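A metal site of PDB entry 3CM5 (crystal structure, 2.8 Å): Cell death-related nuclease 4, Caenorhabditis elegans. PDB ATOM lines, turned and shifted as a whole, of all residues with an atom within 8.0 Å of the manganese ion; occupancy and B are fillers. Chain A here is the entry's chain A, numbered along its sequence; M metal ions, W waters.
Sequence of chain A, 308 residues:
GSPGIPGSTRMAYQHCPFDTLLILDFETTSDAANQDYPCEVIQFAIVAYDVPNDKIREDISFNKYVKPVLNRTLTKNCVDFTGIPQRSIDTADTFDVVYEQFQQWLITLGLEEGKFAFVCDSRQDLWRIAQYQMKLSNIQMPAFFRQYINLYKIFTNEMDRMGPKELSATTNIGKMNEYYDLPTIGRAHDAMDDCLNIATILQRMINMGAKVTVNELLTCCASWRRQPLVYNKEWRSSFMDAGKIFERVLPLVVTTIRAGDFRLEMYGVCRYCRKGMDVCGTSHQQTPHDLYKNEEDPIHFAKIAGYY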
ATOM      1  N   LEU A  24       9.864 -18.698  10.093  1.00  0.00           N
ATOM      2  CA  LEU A  24       9.109 -18.279   8.914  1.00  0.00           C
ATOM      3  C   LEU A  24       9.990 -17.507   7.946  1.00  0.00           C
ATOM      4  O   LEU A  24      10.782 -16.657   8.356  1.00  0.00           O
ATOM      5  CB  LEU A  24       7.958 -17.373   9.361  1.00  0.00           C
ATOM      6  CG  LEU A  24       6.922 -16.704   8.460  1.00  0.00           C
ATOM      7  CD1 LEU A  24       5.970 -15.940   9.353  1.00  0.00           C
ATOM      8  CD2 LEU A  24       7.566 -15.711   7.539  1.00  0.00           C
ATOM      9  N   ASP A  25       9.868 -17.800   6.654  1.00  0.00           N
ATOM     10  CA  ASP A  25      10.472 -16.919   5.653  1.00  0.00           C
ATOM     11  C   ASP A  25       9.581 -16.859   4.447  1.00  0.00           C
ATOM     12  O   ASP A  25       8.973 -17.862   4.065  1.00  0.00           O
ATOM     13  CB  ASP A  25      11.890 -17.362   5.254  1.00  0.00           C
ATOM     14  CG  ASP A  25      12.639 -16.304   4.459  1.00  0.00           C
ATOM     15  OD1 ASP A  25      12.681 -15.117   4.875  1.00  0.00           O
ATOM     16  OD2 ASP A  25      13.199 -16.644   3.411  1.00  0.00           O
ATOM     17  N   PHE A  26       9.478 -15.665   3.861  1.00  0.00           N
ATOM     18  CA  PHE A  26       8.759 -15.452   2.616  1.00  0.00           C
ATOM     19  C   PHE A  26       9.774 -15.203   1.522  1.00  0.00           C
ATOM     20  O   PHE A  26      10.897 -14.756   1.793  1.00  0.00           O
ATOM     21  CB  PHE A  26       7.901 -14.197   2.693  1.00  0.00           C
ATOM     22  CG  PHE A  26       6.768 -14.268   3.675  1.00  0.00           C
ATOM     23  CD1 PHE A  26       5.719 -15.150   3.495  1.00  0.00           C
ATOM     24  CD2 PHE A  26       6.736 -13.382   4.741  1.00  0.00           C
ATOM     25  CE1 PHE A  26       4.666 -15.191   4.392  1.00  0.00           C
ATOM     26  CE2 PHE A  26       5.672 -13.405   5.645  1.00  0.00           C
ATOM     27  CZ  PHE A  26       4.638 -14.314   5.471  1.00  0.00           C
ATOM     28  N   GLU A  27       9.374 -15.500   0.290  1.00  0.00           N
ATOM     29  CA  GLU A  27      10.020 -14.854  -0.854  1.00  0.00           C
ATOM     30  C   GLU A  27       8.932 -14.086  -1.596  1.00  0.00           C
ATOM     31  O   GLU A  27       7.741 -14.459  -1.542  1.00  0.00           O
ATOM     32  CB  GLU A  27      10.717 -15.852  -1.793  1.00  0.00           C
ATOM     33  CG  GLU A  27      11.679 -16.783  -1.109  1.00  0.00           C
ATOM     34  CD  GLU A  27      12.881 -16.094  -0.542  1.00  0.00           C
ATOM     35  OE1 GLU A  27      13.472 -15.311  -1.299  1.00  0.00           O
ATOM     36  OE2 GLU A  27      13.242 -16.360   0.636  1.00  0.00           O
ATOM     37  N   THR A  28       9.332 -13.009  -2.254  1.00  0.00           N
ATOM     38  CA  THR A  28       8.344 -12.177  -2.928  1.00  0.00           C
ATOM     39  C   THR A  28       8.767 -11.888  -4.325  1.00  0.00           C
ATOM     40  O   THR A  28       9.928 -12.084  -4.661  1.00  0.00           O
ATOM     41  CB  THR A  28       8.210 -10.828  -2.256  1.00  0.00           C
ATOM     42  OG1 THR A  28       9.370 -10.048  -2.553  1.00  0.00           O
ATOM     43  CG2 THR A  28       8.036 -10.986  -0.748  1.00  0.00           C
ATOM     44  N   GLN A  43       6.405 -17.335  -2.201  1.00  0.00           N
ATOM     45  CA  GLN A  43       6.663 -18.556  -1.429  1.00  0.00           C
ATOM     46  C   GLN A  43       6.527 -18.234   0.063  1.00  0.00           C
ATOM     47  O   GLN A  43       6.985 -17.154   0.522  1.00  0.00           O
ATOM     48  CB  GLN A  43       8.049 -19.111  -1.746  1.00  0.00           C
ATOM     49  CG  GLN A  43       8.285 -20.529  -1.240  1.00  0.00           C
ATOM     50  CD  GLN A  43       9.694 -21.057  -1.544  1.00  0.00           C
ATOM     51  OE1 GLN A  43      10.639 -20.308  -1.800  1.00  0.00           O
ATOM     52  NE2 GLN A  43       9.823 -22.374  -1.470  1.00  0.00           N
ATOM     53  N   PHE A  81      17.189 -14.609  -8.660  1.00  0.00           N
ATOM     54  CA  PHE A  81      17.378 -14.537  -7.216  1.00  0.00           C
ATOM     55  C   PHE A  81      16.825 -15.774  -6.492  1.00  0.00           C
ATOM     56  O   PHE A  81      17.561 -16.491  -5.805  1.00  0.00           O
ATOM     57  CB  PHE A  81      16.671 -13.270  -6.726  1.00  0.00           C
ATOM     58  CG  PHE A  81      17.096 -12.804  -5.349  1.00  0.00           C
ATOM     59  CD1 PHE A  81      18.422 -12.474  -5.081  1.00  0.00           C
ATOM     60  CD2 PHE A  81      16.132 -12.651  -4.328  1.00  0.00           C
ATOM     61  CE1 PHE A  81      18.790 -12.020  -3.791  1.00  0.00           C
ATOM     62  CE2 PHE A  81      16.491 -12.189  -3.045  1.00  0.00           C
ATOM     63  CZ  PHE A  81      17.808 -11.881  -2.775  1.00  0.00           C
ATOM     64  N   THR A  82      15.531 -16.026  -6.693  1.00  0.00           N
ATOM     65  CA  THR A  82      14.774 -16.952  -5.877  1.00  0.00           C
ATOM     66  C   THR A  82      14.810 -18.366  -6.433  1.00  0.00           C
ATOM     67  O   THR A  82      14.461 -19.359  -5.716  1.00  0.00           O
ATOM     68  CB  THR A  82      13.303 -16.508  -5.744  1.00  0.00           C
ATOM     69  OG1 THR A  82      12.661 -16.544  -7.028  1.00  0.00           O
ATOM     70  CG2 THR A  82      13.221 -15.105  -5.177  1.00  0.00           C
ATOM     71  N   ASP A 121      14.710 -13.960   9.921  1.00  0.00           N
ATOM     72  CA  ASP A 121      16.104 -13.609   9.728  1.00  0.00           C
ATOM     73  C   ASP A 121      16.310 -12.113   9.857  1.00  0.00           C
ATOM     74  O   ASP A 121      17.456 -11.659   9.927  1.00  0.00           O
ATOM     75  CB  ASP A 121      16.599 -14.075   8.354  1.00  0.00           C
ATOM     76  CG  ASP A 121      16.111 -13.182   7.252  1.00  0.00           C
ATOM     77  OD1 ASP A 121      14.891 -13.179   6.992  1.00  0.00           O
ATOM     78  OD2 ASP A 121      16.943 -12.446   6.680  1.00  0.00           O
ATOM     79  N   ASP A 125      10.592  -9.936   6.815  1.00  0.00           N
ATOM     80  CA  ASP A 125       9.510 -10.878   6.673  1.00  0.00           C
ATOM     81  C   ASP A 125       8.207 -10.410   7.274  1.00  0.00           C
ATOM     82  O   ASP A 125       7.168 -10.525   6.630  1.00  0.00           O
ATOM     83  CB  ASP A 125       9.916 -12.216   7.255  1.00  0.00           C
ATOM     84  CG  ASP A 125      10.895 -12.932   6.380  1.00  0.00           C
ATOM     85  OD1 ASP A 125      10.454 -13.478   5.340  1.00  0.00           O
ATOM     86  OD2 ASP A 125      12.101 -12.939   6.706  1.00  0.00           O
ATOM     87  N   ILE A 129       7.301  -7.319   4.566  1.00  0.00           N
ATOM     88  CA  ILE A 129       6.612  -8.222   3.644  1.00  0.00           C
ATOM     89  C   ILE A 129       5.192  -8.612   4.094  1.00  0.00           C
ATOM     90  O   ILE A 129       4.217  -8.351   3.369  1.00  0.00           O
ATOM     91  CB  ILE A 129       7.462  -9.436   3.333  1.00  0.00           C
ATOM     92  CG1 ILE A 129       8.733  -8.955   2.611  1.00  0.00           C
ATOM     93  CG2 ILE A 129       6.654 -10.410   2.521  1.00  0.00           C
ATOM     94  CD1 ILE A 129       9.834  -9.999   2.460  1.00  0.00           C
ATOM     95  N   ILE A 173      21.465 -14.486   6.902  1.00  0.00           N
ATOM     96  CA  ILE A 173      21.727 -15.906   7.051  1.00  0.00           C
ATOM     97  C   ILE A 173      23.214 -16.221   6.786  1.00  0.00           C
ATOM     98  O   ILE A 173      23.915 -16.681   7.680  1.00  0.00           O
ATOM     99  CB  ILE A 173      20.797 -16.763   6.163  1.00  0.00           C
ATOM    100  CG1 ILE A 173      19.334 -16.484   6.518  1.00  0.00           C
ATOM    101  CG2 ILE A 173      21.152 -18.242   6.297  1.00  0.00           C
ATOM    102  CD1 ILE A 173      18.343 -17.264   5.714  1.00  0.00           C
ATOM    103  N   ARG A 187      19.801 -24.291  -1.176  1.00  0.00           N
ATOM    104  CA  ARG A 187      19.991 -23.108  -2.022  1.00  0.00           C
ATOM    105  C   ARG A 187      19.488 -21.804  -1.360  1.00  0.00           C
ATOM    106  O   ARG A 187      18.367 -21.765  -0.841  1.00  0.00           O
ATOM    107  CB  ARG A 187      19.219 -23.338  -3.307  1.00  0.00           C
ATOM    108  CG  ARG A 187      19.978 -23.065  -4.592  1.00  0.00           C
ATOM    109  CD  ARG A 187      19.060 -23.320  -5.792  1.00  0.00           C
ATOM    110  NE  ARG A 187      17.647 -23.008  -5.520  1.00  0.00           N
ATOM    111  CZ  ARG A 187      17.091 -21.783  -5.477  1.00  0.00           C
ATOM    112  NH1 ARG A 187      17.826 -20.674  -5.661  1.00  0.00           N
ATOM    113  NH2 ARG A 187      15.777 -21.684  -5.233  1.00  0.00           N
ATOM    114  N   ALA A 188      20.300 -20.750  -1.402  1.00  0.00           N
ATOM    115  CA  ALA A 188      19.903 -19.431  -0.898  1.00  0.00           C
ATOM    116  C   ALA A 188      18.639 -18.910  -1.572  1.00  0.00           C
ATOM    117  O   ALA A 188      18.486 -19.016  -2.785  1.00  0.00           O
ATOM    118  CB  ALA A 188      21.009 -18.449  -1.107  1.00  0.00           C
ATOM    119  N   HIS A 189      17.726 -18.352  -0.779  1.00  0.00           N
ATOM    120  CA  HIS A 189      16.520 -17.685  -1.311  1.00  0.00           C
ATOM    121  C   HIS A 189      15.377 -18.577  -1.753  1.00  0.00           C
ATOM    122  O   HIS A 189      14.358 -18.093  -2.235  1.00  0.00           O
ATOM    123  CB  HIS A 189      16.906 -16.720  -2.407  1.00  0.00           C
ATOM    124  CG  HIS A 189      17.899 -15.710  -1.946  1.00  0.00           C
ATOM    125  ND1 HIS A 189      17.648 -14.856  -0.896  1.00  0.00           N
ATOM    126  CD2 HIS A 189      19.164 -15.450  -2.353  1.00  0.00           C
ATOM    127  CE1 HIS A 189      18.698 -14.096  -0.686  1.00  0.00           C
ATOM    128  NE2 HIS A 189      19.639 -14.431  -1.554  1.00  0.00           N
ATOM    129  N   ASP A 190      15.533 -19.887  -1.603  1.00  0.00           N
ATOM    130  CA  ASP A 190      14.375 -20.737  -1.462  1.00  0.00           C
ATOM    131  C   ASP A 190      13.894 -20.546  -0.015  1.00  0.00           C
ATOM    132  O   ASP A 190      14.655 -20.746   0.927  1.00  0.00           O
ATOM    133  CB  ASP A 190      14.745 -22.188  -1.727  1.00  0.00           C
ATOM    134  CG  ASP A 190      13.581 -23.101  -1.500  1.00  0.00           C
ATOM    135  OD1 ASP A 190      13.188 -23.267  -0.327  1.00  0.00           O
ATOM    136  OD2 ASP A 190      13.027 -23.633  -2.474  1.00  0.00           O
ATOM    137  N   ALA A 191      12.639 -20.134   0.170  1.00  0.00           N
ATOM    138  CA  ALA A 191      12.162 -19.787   1.508  1.00  0.00           C
ATOM    139  C   ALA A 191      12.277 -20.941   2.491  1.00  0.00           C
ATOM    140  O   ALA A 191      12.613 -20.730   3.665  1.00  0.00           O
ATOM    141  CB  ALA A 191      10.741 -19.248   1.480  1.00  0.00           C
ATOM    142  N   MET A 192      11.989 -22.155   2.026  1.00  0.00           N
ATOM    143  CA  MET A 192      12.109 -23.317   2.880  1.00  0.00           C
ATOM    144  C   MET A 192      13.567 -23.552   3.221  1.00  0.00           C
ATOM    145  O   MET A 192      13.883 -23.726   4.380  1.00  0.00           O
ATOM    146  CB  MET A 192      11.480 -24.548   2.240  1.00  0.00           C
ATOM    147  CG  MET A 192      11.614 -25.809   3.072  1.00  0.00           C
ATOM    148  SD  MET A 192      10.886 -25.637   4.719  1.00  0.00           S
ATOM    149  CE  MET A 192       9.147 -25.796   4.357  1.00  0.00           C
ATOM    150  N   ASP A 193      14.441 -23.532   2.227  1.00  0.00           N
ATOM    151  CA  ASP A 193      15.858 -23.674   2.513  1.00  0.00           C
ATOM    152  C   ASP A 193      16.358 -22.579   3.465  1.00  0.00           C
ATOM    153  O   ASP A 193      17.130 -22.869   4.372  1.00  0.00           O
ATOM    154  CB  ASP A 193      16.702 -23.699   1.238  1.00  0.00           C
ATOM    155  CG  ASP A 193      16.719 -25.085   0.557  1.00  0.00           C
ATOM    156  OD1 ASP A 193      16.182 -26.080   1.120  1.00  0.00           O
ATOM    157  OD2 ASP A 193      17.291 -25.165  -0.573  1.00  0.00           O
ATOM    158  N   ASP A 194      15.889 -21.352   3.266  1.00  0.00           N
ATOM    159  CA  ASP A 194      16.189 -20.253   4.200  1.00  0.00           C
ATOM    160  C   ASP A 194      15.748 -20.638   5.628  1.00  0.00           C
ATOM    161  O   ASP A 194      16.496 -20.431   6.602  1.00  0.00           O
ATOM    162  CB  ASP A 194      15.512 -18.949   3.756  1.00  0.00           C
ATOM    163  CG  ASP A 194      16.157 -18.312   2.491  1.00  0.00           C
ATOM    164  OD1 ASP A 194      17.310 -18.643   2.122  1.00  0.00           O
ATOM    165  OD2 ASP A 194      15.476 -17.460   1.875  1.00  0.00           O
ATOM    166  N   CYS A 195      14.532 -21.193   5.742  1.00  0.00           N
ATOM    167  CA  CYS A 195      13.987 -21.622   7.038  1.00  0.00           C
ATOM    168  C   CYS A 195      14.839 -22.681   7.712  1.00  0.00           C
ATOM    169  O   CYS A 195      15.085 -22.605   8.918  1.00  0.00           O
ATOM    170  CB  CYS A 195      12.561 -22.151   6.909  1.00  0.00           C
ATOM    171  SG  CYS A 195      11.306 -20.865   6.879  1.00  0.00           S
ATOM    172  N   ILE A 198      17.968 -21.137   9.141  1.00  0.00           N
ATOM    173  CA  ILE A 198      17.672 -20.376  10.330  1.00  0.00           C
ATOM    174  C   ILE A 198      17.399 -21.274  11.558  1.00  0.00           C
ATOM    175  O   ILE A 198      17.873 -20.999  12.662  1.00  0.00           O
ATOM    176  CB  ILE A 198      16.537 -19.408  10.073  1.00  0.00           C
ATOM    177  CG1 ILE A 198      16.978 -18.389   9.007  1.00  0.00           C
ATOM    178  CG2 ILE A 198      16.095 -18.703  11.369  1.00  0.00           C
ATOM    179  CD1 ILE A 198      15.796 -17.654   8.352  1.00  0.00           C
HETATM  180 MN    MN M   1      14.424 -15.748   2.135  1.00  0.00          MN
HETATM  181  O   HOH W   1      13.283 -13.586   2.660  1.00  0.00           O
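The manganese ion is bound by the side-chain carboxylate (OD2) of Asp 25 (2.0 Å).
OE2 of Glu 27 binds the manganese ion (2.0 Å).
The manganese ion is bound by OD2 of Asp 194.
Water W1 is bound to the manganese ion (2.5 Å).
The manganese ion has four donor atoms within binding distance.
Water W1 bridges OD1 of Asp 25 (2.8 Å) and O of Phe 26 (2.8 Å).
O of Phe 26 touches the manganese ion (3.7 Å).
The nearest printed residue that does not touch the manganese ion is His 189 (4.5 Å).
SG of Cys 195 sits at hydrogen-bond distance from N of Asp 25 (3.4 Å).
The backbone NH (N) of Glu 27 is in hydrogen-bond range of the backbone carbonyl oxygen (O) of Gln 43 (2.9 Å).
OD1 of Asp 194 is in hydrogen-bond range of N of His 189, at 2.9 Å.
The backbone NH (N) of Phe 26 is in hydrogen-bond range of the side-chain carboxylate (OD1) of Asp 125, 2.8 Å away.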
